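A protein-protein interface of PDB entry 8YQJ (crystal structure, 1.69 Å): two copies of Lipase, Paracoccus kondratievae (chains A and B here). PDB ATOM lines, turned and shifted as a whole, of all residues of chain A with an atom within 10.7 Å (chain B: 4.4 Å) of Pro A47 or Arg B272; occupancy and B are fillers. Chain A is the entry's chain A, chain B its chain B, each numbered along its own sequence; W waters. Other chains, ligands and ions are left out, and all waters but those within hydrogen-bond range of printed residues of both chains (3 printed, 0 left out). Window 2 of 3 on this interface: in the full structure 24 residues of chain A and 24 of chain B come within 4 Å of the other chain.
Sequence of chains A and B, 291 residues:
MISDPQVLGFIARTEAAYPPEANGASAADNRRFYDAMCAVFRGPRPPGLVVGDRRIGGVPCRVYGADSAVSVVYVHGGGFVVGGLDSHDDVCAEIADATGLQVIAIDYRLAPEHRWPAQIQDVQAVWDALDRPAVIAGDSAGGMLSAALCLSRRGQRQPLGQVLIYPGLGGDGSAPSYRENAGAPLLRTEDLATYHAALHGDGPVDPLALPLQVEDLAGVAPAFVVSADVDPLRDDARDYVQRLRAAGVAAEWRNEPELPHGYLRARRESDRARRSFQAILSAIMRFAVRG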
ATOM      1  N   GLY A  43     -16.334 -15.021   4.879  1.00  0.00           N
ATOM      2  CA  GLY A  43     -15.728 -13.894   4.217  1.00  0.00           C
ATOM      3  C   GLY A  43     -16.435 -12.597   4.545  1.00  0.00           C
ATOM      4  O   GLY A  43     -17.532 -12.556   5.132  1.00  0.00           O
ATOM      5  N   PRO A  44     -15.813 -11.497   4.144  1.00  0.00           N
ATOM      6  CA  PRO A  44     -16.371 -10.179   4.441  1.00  0.00           C
ATOM      7  C   PRO A  44     -17.446  -9.793   3.436  1.00  0.00           C
ATOM      8  O   PRO A  44     -17.537 -10.330   2.327  1.00  0.00           O
ATOM      9  CB  PRO A  44     -15.151  -9.259   4.333  1.00  0.00           C
ATOM     10  CG  PRO A  44     -14.310  -9.922   3.309  1.00  0.00           C
ATOM     11  CD  PRO A  44     -14.493 -11.405   3.499  1.00  0.00           C
ATOM     12  N   ARG A  45     -18.287  -8.863   3.867  1.00  0.00           N
ATOM     13  CA  ARG A  45     -19.250  -8.245   2.973  1.00  0.00           C
ATOM     14  C   ARG A  45     -18.549  -7.348   1.958  1.00  0.00           C
ATOM     15  O   ARG A  45     -17.531  -6.718   2.268  1.00  0.00           O
ATOM     16  CB  ARG A  45     -20.224  -7.393   3.767  1.00  0.00           C
ATOM     17  CG  ARG A  45     -21.234  -8.176   4.504  1.00  0.00           C
ATOM     18  CD  ARG A  45     -22.322  -7.271   4.960  1.00  0.00           C
ATOM     19  NE  ARG A  45     -23.292  -8.033   5.715  1.00  0.00           N
ATOM     20  CZ  ARG A  45     -24.179  -7.507   6.544  1.00  0.00           C
ATOM     21  NH1 ARG A  45     -24.215  -6.206   6.774  1.00  0.00           N
ATOM     22  NH2 ARG A  45     -25.070  -8.308   7.130  1.00  0.00           N
ATOM     23  N   PRO A  46     -19.089  -7.234   0.752  1.00  0.00           N
ATOM     24  CA  PRO A  46     -18.663  -6.152  -0.128  1.00  0.00           C
ATOM     25  C   PRO A  46     -18.982  -4.818   0.524  1.00  0.00           C
ATOM     26  O   PRO A  46     -20.128  -4.572   0.918  1.00  0.00           O
ATOM     27  CB  PRO A  46     -19.494  -6.378  -1.400  1.00  0.00           C
ATOM     28  CG  PRO A  46     -19.792  -7.825  -1.384  1.00  0.00           C
ATOM     29  CD  PRO A  46     -20.022  -8.151   0.071  1.00  0.00           C
ATOM     30  N   PRO A  47     -17.988  -3.950   0.682  1.00  0.00           N
ATOM     31  CA  PRO A  47     -18.193  -2.737   1.494  1.00  0.00           C
ATOM     32  C   PRO A  47     -19.242  -1.781   0.945  1.00  0.00           C
ATOM     33  O   PRO A  47     -19.867  -1.057   1.730  1.00  0.00           O
ATOM     34  CB  PRO A  47     -16.797  -2.099   1.517  1.00  0.00           C
ATOM     35  CG  PRO A  47     -16.120  -2.630   0.269  1.00  0.00           C
ATOM     36  CD  PRO A  47     -16.655  -4.014   0.062  1.00  0.00           C
ATOM     37  N   GLY A  48     -19.463  -1.744  -0.359  1.00  0.00           N
ATOM     38  CA  GLY A  48     -20.460  -0.814  -0.846  1.00  0.00           C
ATOM     39  C   GLY A  48     -21.867  -1.354  -0.893  1.00  0.00           C
ATOM     40  O   GLY A  48     -22.798  -0.626  -1.244  1.00  0.00           O
ATOM     41  N   LEU A  49     -22.058  -2.617  -0.533  1.00  0.00           N
ATOM     42  CA  LEU A  49     -23.345  -3.275  -0.712  1.00  0.00           C
ATOM     43  C   LEU A  49     -24.325  -2.852   0.375  1.00  0.00           C
ATOM     44  O   LEU A  49     -24.028  -2.964   1.568  1.00  0.00           O
ATOM     45  CB  LEU A  49     -23.156  -4.788  -0.691  1.00  0.00           C
ATOM     46  CG  LEU A  49     -24.429  -5.615  -0.887  1.00  0.00           C
ATOM     47  CD1 LEU A  49     -24.901  -5.560  -2.321  1.00  0.00           C
ATOM     48  CD2 LEU A  49     -24.147  -7.075  -0.525  1.00  0.00           C
ATOM     49  N   VAL A  50     -25.491  -2.362  -0.044  1.00  0.00           N
ATOM     50  CA  VAL A  50     -26.554  -2.033   0.905  1.00  0.00           C
ATOM     51  C   VAL A  50     -27.159  -3.321   1.445  1.00  0.00           C
ATOM     52  O   VAL A  50     -27.508  -4.229   0.680  1.00  0.00           O
ATOM     53  CB  VAL A  50     -27.611  -1.137   0.237  1.00  0.00           C
ATOM     54  CG1 VAL A  50     -26.955   0.138  -0.299  1.00  0.00           C
ATOM     55  CG2 VAL A  50     -28.336  -1.874  -0.903  1.00  0.00           C
ATOM     56  N   VAL A  51     -27.260  -3.415   2.775  1.00  0.00           N
ATOM     57  CA  VAL A  51     -27.792  -4.585   3.469  1.00  0.00           C
ATOM     58  C   VAL A  51     -28.725  -4.111   4.572  1.00  0.00           C
ATOM     59  O   VAL A  51     -28.354  -3.228   5.356  1.00  0.00           O
ATOM     60  CB  VAL A  51     -26.674  -5.462   4.070  1.00  0.00           C
ATOM     61  CG1 VAL A  51     -27.271  -6.697   4.728  1.00  0.00           C
ATOM     62  CG2 VAL A  51     -25.688  -5.892   2.987  1.00  0.00           C
ATOM     63  N   TYR A  64     -30.062  -7.967   0.575  1.00  0.00           N
ATOM     64  CA  TYR A  64     -28.764  -7.567   0.035  1.00  0.00           C
ATOM     65  C   TYR A  64     -28.935  -6.960  -1.350  1.00  0.00           C
ATOM     66  O   TYR A  64     -29.496  -7.603  -2.242  1.00  0.00           O
ATOM     67  CB  TYR A  64     -27.797  -8.746  -0.083  1.00  0.00           C
ATOM     68  CG  TYR A  64     -27.578  -9.582   1.151  1.00  0.00           C
ATOM     69  CD1 TYR A  64     -28.497 -10.550   1.534  1.00  0.00           C
ATOM     70  CD2 TYR A  64     -26.430  -9.431   1.912  1.00  0.00           C
ATOM     71  CE1 TYR A  64     -28.291 -11.327   2.646  1.00  0.00           C
ATOM     72  CE2 TYR A  64     -26.209 -10.208   3.033  1.00  0.00           C
ATOM     73  CZ  TYR A  64     -27.146 -11.160   3.383  1.00  0.00           C
ATOM     74  OH  TYR A  64     -26.950 -11.952   4.475  1.00  0.00           O
ATOM     75  N   GLY A  65     -28.416  -5.746  -1.529  1.00  0.00           N
ATOM     76  CA  GLY A  65     -28.416  -5.068  -2.807  1.00  0.00           C
ATOM     77  C   GLY A  65     -29.659  -4.228  -3.023  1.00  0.00           C
ATOM     78  O   GLY A  65     -30.658  -4.327  -2.306  1.00  0.00           O
ATOM     79  N   ASP A  89     -24.037 -15.164   5.818  1.00  0.00           N
ATOM     80  CA  ASP A  89     -24.081 -13.779   5.361  1.00  0.00           C
ATOM     81  C   ASP A  89     -23.218 -13.557   4.123  1.00  0.00           C
ATOM     82  O   ASP A  89     -23.613 -12.847   3.184  1.00  0.00           O
ATOM     83  CB  ASP A  89     -23.636 -12.864   6.506  1.00  0.00           C
ATOM     84  CG  ASP A  89     -23.787 -11.402   6.162  1.00  0.00           C
ATOM     85  OD1 ASP A  89     -24.934 -10.904   6.160  1.00  0.00           O
ATOM     86  OD2 ASP A  89     -22.767 -10.754   5.880  1.00  0.00           O
ATOM     87  N   ASP A  90     -22.038 -14.156   4.096  1.00  0.00           N
ATOM     88  CA  ASP A  90     -21.102 -13.840   3.033  1.00  0.00           C
ATOM     89  C   ASP A  90     -21.548 -14.465   1.724  1.00  0.00           C
ATOM     90  O   ASP A  90     -21.365 -13.876   0.655  1.00  0.00           O
ATOM     91  CB  ASP A  90     -19.707 -14.310   3.446  1.00  0.00           C
ATOM     92  CG  ASP A  90     -19.661 -15.786   3.816  1.00  0.00           C
ATOM     93  OD1 ASP A  90     -20.651 -16.349   4.351  1.00  0.00           O
ATOM     94  OD2 ASP A  90     -18.592 -16.397   3.606  1.00  0.00           O
ATOM     95  N   ALA A  93     -24.369 -12.210   0.402  1.00  0.00           N
ATOM     96  CA  ALA A  93     -23.802 -10.947  -0.060  1.00  0.00           C
ATOM     97  C   ALA A  93     -23.021 -11.131  -1.354  1.00  0.00           C
ATOM     98  O   ALA A  93     -23.108 -10.301  -2.264  1.00  0.00           O
ATOM     99  CB  ALA A  93     -22.919 -10.345   1.018  1.00  0.00           C
ATOM    100  N   GLU A  94     -22.269 -12.226  -1.464  1.00  0.00           N
ATOM    101  CA  GLU A  94     -21.525 -12.449  -2.695  1.00  0.00           C
ATOM    102  C   GLU A  94     -22.458 -12.747  -3.867  1.00  0.00           C
ATOM    103  O   GLU A  94     -22.145 -12.382  -5.007  1.00  0.00           O
ATOM    104  CB  GLU A  94     -20.493 -13.562  -2.488  1.00  0.00           C
ATOM    105  CG  GLU A  94     -19.341 -13.085  -1.628  1.00  0.00           C
ATOM    106  CD  GLU A  94     -18.227 -14.109  -1.489  1.00  0.00           C
ATOM    107  OE1 GLU A  94     -18.149 -15.021  -2.334  1.00  0.00           O
ATOM    108  OE2 GLU A  94     -17.458 -14.012  -0.515  1.00  0.00           O
ATOM    109  N   ALA A  96     -25.504 -11.357  -4.320  1.00  0.00           N
ATOM    110  CA  ALA A  96     -25.985 -10.047  -4.737  1.00  0.00           C
ATOM    111  C   ALA A  96     -24.890  -9.243  -5.432  1.00  0.00           C
ATOM    112  O   ALA A  96     -25.131  -8.617  -6.472  1.00  0.00           O
ATOM    113  CB  ALA A  96     -26.508  -9.272  -3.525  1.00  0.00           C
ATOM    114  N   ASP A  97     -23.675  -9.262  -4.880  1.00  0.00           N
ATOM    115  CA  ASP A  97     -22.575  -8.521  -5.483  1.00  0.00           C
ATOM    116  C   ASP A  97     -22.249  -9.033  -6.880  1.00  0.00           C
ATOM    117  O   ASP A  97     -21.992  -8.243  -7.793  1.00  0.00           O
ATOM    118  CB  ASP A  97     -21.344  -8.606  -4.580  1.00  0.00           C
ATOM    119  CG  ASP A  97     -20.185  -7.778  -5.090  1.00  0.00           C
ATOM    120  OD1 ASP A  97     -20.251  -6.537  -5.022  1.00  0.00           O
ATOM    121  OD2 ASP A  97     -19.191  -8.387  -5.535  1.00  0.00           O
ATOM    122  N   ALA A  98     -22.259 -10.350  -7.068  1.00  0.00           N
ATOM    123  CA  ALA A  98     -21.780 -10.884  -8.333  1.00  0.00           C
ATOM    124  C   ALA A  98     -22.831 -10.725  -9.420  1.00  0.00           C
ATOM    125  O   ALA A  98     -22.495 -10.399 -10.561  1.00  0.00           O
ATOM    126  CB  ALA A  98     -21.379 -12.352  -8.177  1.00  0.00           C
ATOM    127  N   ARG A 267     -14.689 -22.036  -0.265  1.00  0.00           N
ATOM    128  CA  ARG A 267     -14.405 -21.343  -1.521  1.00  0.00           C
ATOM    129  C   ARG A 267     -13.308 -20.297  -1.391  1.00  0.00           C
ATOM    130  O   ARG A 267     -12.823 -19.792  -2.411  1.00  0.00           O
ATOM    131  CB  ARG A 267     -15.673 -20.675  -2.042  1.00  0.00           C
ATOM    132  CG  ARG A 267     -16.039 -19.420  -1.246  1.00  0.00           C
ATOM    133  CD  ARG A 267     -17.451 -18.978  -1.529  1.00  0.00           C
ATOM    134  NE  ARG A 267     -17.758 -17.740  -0.820  1.00  0.00           N
ATOM    135  CZ  ARG A 267     -18.045 -17.662   0.471  1.00  0.00           C
ATOM    136  NH1 ARG A 267     -18.116 -18.743   1.233  1.00  0.00           N
ATOM    137  NH2 ARG A 267     -18.255 -16.466   1.017  1.00  0.00           N
ATOM    138  N   ARG A 268     -12.940 -19.918  -0.180  1.00  0.00           N
ATOM    139  CA  ARG A 268     -11.866 -18.959  -0.016  1.00  0.00           C
ATOM    140  C   ARG A 268     -10.507 -19.632   0.085  1.00  0.00           C
ATOM    141  O   ARG A 268      -9.477 -18.942   0.108  1.00  0.00           O
ATOM    142  CB  ARG A 268     -12.128 -18.102   1.220  1.00  0.00           C
ATOM    143  CG  ARG A 268     -13.423 -17.320   1.119  1.00  0.00           C
ATOM    144  CD  ARG A 268     -13.726 -16.662   2.459  1.00  0.00           C
ATOM    145  NE  ARG A 268     -12.850 -15.528   2.736  1.00  0.00           N
ATOM    146  CZ  ARG A 268     -12.307 -15.268   3.918  1.00  0.00           C
ATOM    147  NH1 ARG A 268     -12.446 -16.093   4.945  1.00  0.00           N
ATOM    148  NH2 ARG A 268     -11.635 -14.131   4.086  1.00  0.00           N
ATOM    149  N   ARG A 274     -14.007 -22.932  -4.883  1.00  0.00           N
ATOM    150  CA  ARG A 274     -14.153 -21.639  -5.543  1.00  0.00           C
ATOM    151  C   ARG A 274     -14.800 -21.786  -6.926  1.00  0.00           C
ATOM    152  O   ARG A 274     -15.731 -21.042  -7.264  1.00  0.00           O
ATOM    153  CB  ARG A 274     -12.798 -20.946  -5.616  1.00  0.00           C
ATOM    154  CG  ARG A 274     -12.891 -19.559  -6.201  1.00  0.00           C
ATOM    155  CD  ARG A 274     -11.562 -18.870  -6.141  1.00  0.00           C
ATOM    156  NE  ARG A 274     -10.540 -19.703  -6.762  1.00  0.00           N
ATOM    157  CZ  ARG A 274     -10.358 -19.794  -8.069  1.00  0.00           C
ATOM    158  NH1 ARG A 274     -11.116 -19.126  -8.920  1.00  0.00           N
ATOM    159  NH2 ARG A 274      -9.375 -20.557  -8.533  1.00  0.00           N
ATOM    160  N   GLN A 278     -18.426 -20.433  -8.352  1.00  0.00           N
ATOM    161  CA  GLN A 278     -18.467 -19.704  -9.612  1.00  0.00           C
ATOM    162  C   GLN A 278     -19.535 -20.281 -10.532  1.00  0.00           C
ATOM    163  O   GLN A 278     -20.281 -19.535 -11.162  1.00  0.00           O
ATOM    164  CB  GLN A 278     -17.085 -19.709 -10.271  1.00  0.00           C
ATOM    165  CG  GLN A 278     -16.165 -18.668  -9.621  1.00  0.00           C
ATOM    166  CD  GLN A 278     -14.714 -18.795 -10.009  1.00  0.00           C
ATOM    167  OE1 GLN A 278     -13.868 -18.123  -9.424  1.00  0.00           O
ATOM    168  NE2 GLN A 278     -14.413 -19.677 -10.961  1.00  0.00           N
ATOM    169  N   ASP B   4      -6.102  -2.988   2.176  1.00  0.00           N
ATOM    170  CA  ASP B   4      -6.541  -4.371   2.329  1.00  0.00           C
ATOM    171  C   ASP B   4      -5.309  -5.264   2.432  1.00  0.00           C
ATOM    172  O   ASP B   4      -4.505  -5.298   1.491  1.00  0.00           O
ATOM    173  CB  ASP B   4      -7.420  -4.752   1.131  1.00  0.00           C
ATOM    174  CG  ASP B   4      -8.012  -6.158   1.227  1.00  0.00           C
ATOM    175  OD1 ASP B   4      -7.383  -7.094   1.771  1.00  0.00           O
ATOM    176  OD2 ASP B   4      -9.129  -6.327   0.714  1.00  0.00           O
ATOM    177  N   PRO B 257     -12.724  -1.048  -5.638  1.00  0.00           N
ATOM    178  CA  PRO B 257     -11.897  -0.373  -4.630  1.00  0.00           C
ATOM    179  C   PRO B 257     -10.779  -1.292  -4.154  1.00  0.00           C
ATOM    180  O   PRO B 257     -10.962  -2.500  -4.015  1.00  0.00           O
ATOM    181  CB  PRO B 257     -12.887  -0.075  -3.501  1.00  0.00           C
ATOM    182  CG  PRO B 257     -14.231  -0.077  -4.183  1.00  0.00           C
ATOM    183  CD  PRO B 257     -14.129  -1.155  -5.225  1.00  0.00           C
ATOM    184  N   GLU B 258      -9.620  -0.695  -3.905  1.00  0.00           N
ATOM    185  CA  GLU B 258      -8.473  -1.333  -3.275  1.00  0.00           C
ATOM    186  C   GLU B 258      -7.759  -2.322  -4.184  1.00  0.00           C
ATOM    187  O   GLU B 258      -6.870  -3.035  -3.724  1.00  0.00           O
ATOM    188  CB  GLU B 258      -8.865  -2.071  -1.986  1.00  0.00           C
ATOM    189  CG  GLU B 258      -9.552  -1.216  -0.928  1.00  0.00           C
ATOM    190  CD  GLU B 258      -8.589  -0.275  -0.245  1.00  0.00           C
ATOM    191  OE1 GLU B 258      -7.443  -0.701  -0.005  1.00  0.00           O
ATOM    192  OE2 GLU B 258      -8.991   0.871   0.088  1.00  0.00           O
ATOM    193  N   LEU B 259      -8.118  -2.396  -5.437  1.00  0.00           N
ATOM    194  CA  LEU B 259      -7.450  -3.394  -6.243  1.00  0.00           C
ATOM    195  C   LEU B 259      -6.546  -2.719  -7.264  1.00  0.00           C
ATOM    196  O   LEU B 259      -6.909  -1.668  -7.801  1.00  0.00           O
ATOM    197  CB  LEU B 259      -8.466  -4.281  -6.978  1.00  0.00           C
ATOM    198  CG  LEU B 259      -9.233  -5.292  -6.128  1.00  0.00           C
ATOM    199  CD1 LEU B 259     -10.083  -6.161  -7.027  1.00  0.00           C
ATOM    200  CD2 LEU B 259      -8.237  -6.145  -5.371  1.00  0.00           C
ATOM    201  N   SER B 270      -7.482 -13.133  -2.633  1.00  0.00           N
ATOM    202  CA  SER B 270      -8.086 -11.865  -2.237  1.00  0.00           C
ATOM    203  C   SER B 270      -9.594 -11.965  -2.384  1.00  0.00           C
ATOM    204  O   SER B 270     -10.086 -12.298  -3.463  1.00  0.00           O
ATOM    205  CB  SER B 270      -7.556 -10.706  -3.100  1.00  0.00           C
ATOM    206  OG  SER B 270      -8.426  -9.575  -3.035  1.00  0.00           O
ATOM    207  N   ASP B 271     -10.335 -11.640  -1.315  1.00  0.00           N
ATOM    208  CA  ASP B 271     -11.792 -11.682  -1.416  1.00  0.00           C
ATOM    209  C   ASP B 271     -12.315 -10.684  -2.435  1.00  0.00           C
ATOM    210  O   ASP B 271     -13.275 -10.976  -3.168  1.00  0.00           O
ATOM    211  CB  ASP B 271     -12.440 -11.409  -0.064  1.00  0.00           C
ATOM    212  CG  ASP B 271     -12.183 -12.510   0.936  1.00  0.00           C
ATOM    213  OD1 ASP B 271     -12.635 -13.651   0.697  1.00  0.00           O
ATOM    214  OD2 ASP B 271     -11.608 -12.222   1.997  1.00  0.00           O
ATOM    215  N   ARG B 272     -11.730  -9.480  -2.459  1.00  0.00           N
ATOM    216  CA  ARG B 272     -12.151  -8.461  -3.406  1.00  0.00           C
ATOM    217  C   ARG B 272     -11.936  -8.923  -4.830  1.00  0.00           C
ATOM    218  O   ARG B 272     -12.819  -8.767  -5.683  1.00  0.00           O
ATOM    219  CB  ARG B 272     -11.374  -7.175  -3.156  1.00  0.00           C
ATOM    220  CG  ARG B 272     -11.757  -6.486  -1.854  1.00  0.00           C
ATOM    221  CD  ARG B 272     -11.080  -5.131  -1.803  1.00  0.00           C
ATOM    222  NE  ARG B 272     -11.044  -4.598  -0.447  1.00  0.00           N
ATOM    223  CZ  ARG B 272     -11.892  -3.690   0.013  1.00  0.00           C
ATOM    224  NH1 ARG B 272     -12.904  -3.249  -0.721  1.00  0.00           N
ATOM    225  NH2 ARG B 272     -11.725  -3.217   1.244  1.00  0.00           N
ATOM    226  N   ALA B 273     -10.753  -9.480  -5.106  1.00  0.00           N
ATOM    227  CA  ALA B 273     -10.465  -9.965  -6.450  1.00  0.00           C
ATOM    228  C   ALA B 273     -11.330 -11.164  -6.795  1.00  0.00           C
ATOM    229  O   ALA B 273     -11.810 -11.279  -7.923  1.00  0.00           O
ATOM    230  CB  ALA B 273      -8.981 -10.317  -6.584  1.00  0.00           C
ATOM    231  N   ARG B 274     -11.520 -12.081  -5.841  1.00  0.00           N
ATOM    232  CA  ARG B 274     -12.399 -13.222  -6.068  1.00  0.00           C
ATOM    233  C   ARG B 274     -13.826 -12.763  -6.372  1.00  0.00           C
ATOM    234  O   ARG B 274     -14.478 -13.287  -7.287  1.00  0.00           O
ATOM    235  CB  ARG B 274     -12.366 -14.142  -4.845  1.00  0.00           C
ATOM    236  CG  ARG B 274     -13.177 -15.391  -5.017  1.00  0.00           C
ATOM    237  CD  ARG B 274     -13.069 -16.350  -3.826  1.00  0.00           C
ATOM    238  NE  ARG B 274     -13.324 -15.688  -2.561  1.00  0.00           N
ATOM    239  CZ  ARG B 274     -14.534 -15.380  -2.132  1.00  0.00           C
ATOM    240  NH1 ARG B 274     -15.620 -15.719  -2.816  1.00  0.00           N
ATOM    241  NH2 ARG B 274     -14.660 -14.694  -1.003  1.00  0.00           N
ATOM    242  N   ARG B 275     -14.331 -11.782  -5.624  1.00  0.00           N
ATOM    243  CA  ARG B 275     -15.682 -11.298  -5.899  1.00  0.00           C
ATOM    244  C   ARG B 275     -15.736 -10.614  -7.252  1.00  0.00           C
ATOM    245  O   ARG B 275     -16.751 -10.703  -7.962  1.00  0.00           O
ATOM    246  CB  ARG B 275     -16.158 -10.339  -4.794  1.00  0.00           C
ATOM    247  CG  ARG B 275     -16.460 -11.020  -3.460  1.00  0.00           C
ATOM    248  CD  ARG B 275     -17.243 -10.069  -2.527  1.00  0.00           C
ATOM    249  NE  ARG B 275     -16.630  -8.749  -2.462  1.00  0.00           N
ATOM    250  CZ  ARG B 275     -15.826  -8.330  -1.491  1.00  0.00           C
ATOM    251  NH1 ARG B 275     -15.492  -9.117  -0.478  1.00  0.00           N
ATOM    252  NH2 ARG B 275     -15.360  -7.082  -1.530  1.00  0.00           N
ATOM    253  N   SER B 276     -14.652  -9.941  -7.641  1.00  0.00           N
ATOM    254  CA  SER B 276     -14.658  -9.288  -8.940  1.00  0.00           C
ATOM    255  C   SER B 276     -14.778 -10.320 -10.055  1.00  0.00           C
ATOM    256  O   SER B 276     -15.585 -10.160 -10.976  1.00  0.00           O
ATOM    257  CB  SER B 276     -13.403  -8.443  -9.121  1.00  0.00           C
ATOM    258  OG  SER B 276     -13.515  -7.683 -10.319  1.00  0.00           O
HETATM  259  O   HOH W   1     -13.179 -15.809  -8.302  1.00  0.00           O
HETATM  260  O   HOH W   2     -16.501 -11.851   0.583  1.00  0.00           O
HETATM  261  O   HOH W   3     -17.009  -6.611  -4.190  1.00  0.00           O
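The guanidinium group (NE) of Arg A268 is in salt-bridge range of the side-chain carboxylate (OD1) of Asp B271. OE1 of Glu A94 is in salt-bridge range of NH1 of Arg B274 (2.7 Å).
The guanidinium group (NH1) of Arg A274 lies within hydrogen-bond range of the side-chain amide oxygen (OE1) of Gln A278, at 3.0 Å. The backbone NH (N) of Arg B272 lies close to the side-chain hydroxyl (OG) of Ser B270, 3.4 Å away. The guanidinium group (NH2) of Arg B274 is in salt-bridge range of the side-chain carboxylate (OD1) of Asp B271, at 2.8 Å. The side-chain carboxylate (OD2) of Asp B4 is in salt-bridge range of the guanidinium group (NE) of Arg B272 (2.8 Å). The side-chain carboxylate (OE2) of Glu A94 lies within salt-bridge range of the guanidinium group (NH2) of Arg A267, 3.0 Å away. OD2 of Asp A90 lies within salt-bridge range of NH2 of Arg A267.
Arg A274 touches its own counterpart, Arg B274. Position printed for both chains: 274. Of the 12 pairs that touch across the chains among the printed residues, 1 has its exchanged pair printed and touching as well.
Water W2 lies within hydrogen-bond range of O of Pro A44 (2.5 Å), OE2 of Glu A94 (2.6 Å) and NH1 of Arg B275 (3.1 Å). Water W1 lies within hydrogen-bond range of OE1 of Gln A278 (2.7 Å) and O of Arg B274 (3.0 Å). Water W3 lies within hydrogen-bond range of NE of Arg B275 (2.8 Å) and OD2 of Asp A97 (3.1 Å).
Of the 22 printed residues of chain A, 8 touch a printed residue of chain B. Printed residues of chain A that touch a printed residue of chain B: Pro A44, Pro A46, Pro A47, Glu A94, Asp A97, Arg A267, Arg A268 and Arg A274. Hydrophobic or aromatic side chains of chain A that line the printed part of chain B: Pro A44, Pro A46 and Pro A47. Along chain A the printed residues that touch a printed residue of chain B span positions 44 to 274. Among the printed residues, Asp or Glu carboxylates within 4 Å of a Lys or Arg side-chain nitrogen of the other chain: Glu A94 with Arg B274 (2.7 Å) and Arg A268 with Asp B271 (2.8 Å).
Of the printed residues of chain B, Pro A44 touches Asp B271 (3.4 Å) and Arg B275 (3.7 Å). Printed residues of chain B within 4 Å of Pro A46: Arg B275. Pro A47 touches two residues of chain B. No residue of chain A comes within 4 Å of Pro B257. No residue of chain A comes within 4 Å of Glu B258. Of the printed residues of chain A, Asp B271 touches Pro A44 and Arg A268. Of chain A, only Pro A47 comes within 4 Å of Arg B272. No residue of chain A comes within 4 Å of Ala B273. Printed residues of chain A within 4 Å of Arg B274: Glu A94 (2.7 Å), Arg A267 (3.6 Å), Arg A268 (3.6 Å) and Arg A274 (3.7 Å). Arg B275 touches just these residues of chain A: Pro A44, Pro A46, Pro A47, Glu A94 and Asp A97. No residue of chain A comes within 4 Å of Ser B276. The nearest printed residue of chain B that does not touch Pro A44 is Arg B274 (5.6 Å).
Among the printed residues, merely in contact across the chains: Pro A44 with Asp B271 (3.4 Å), Pro A44 with Arg B275 (3.7 Å), Pro A46 with Arg B275 (3.5 Å), Pro A47 with Arg B272 (3.4 Å), Pro A47 with Arg B275 (3.7 Å), Glu A94 with Arg B275 (3.8 Å), Asp A97 with Arg B275 (3.7 Å), Arg A267 with Arg B274 (3.6 Å), Arg A268 with Arg B274 (3.6 Å) and Arg A274 with Arg B274 (3.7 Å).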
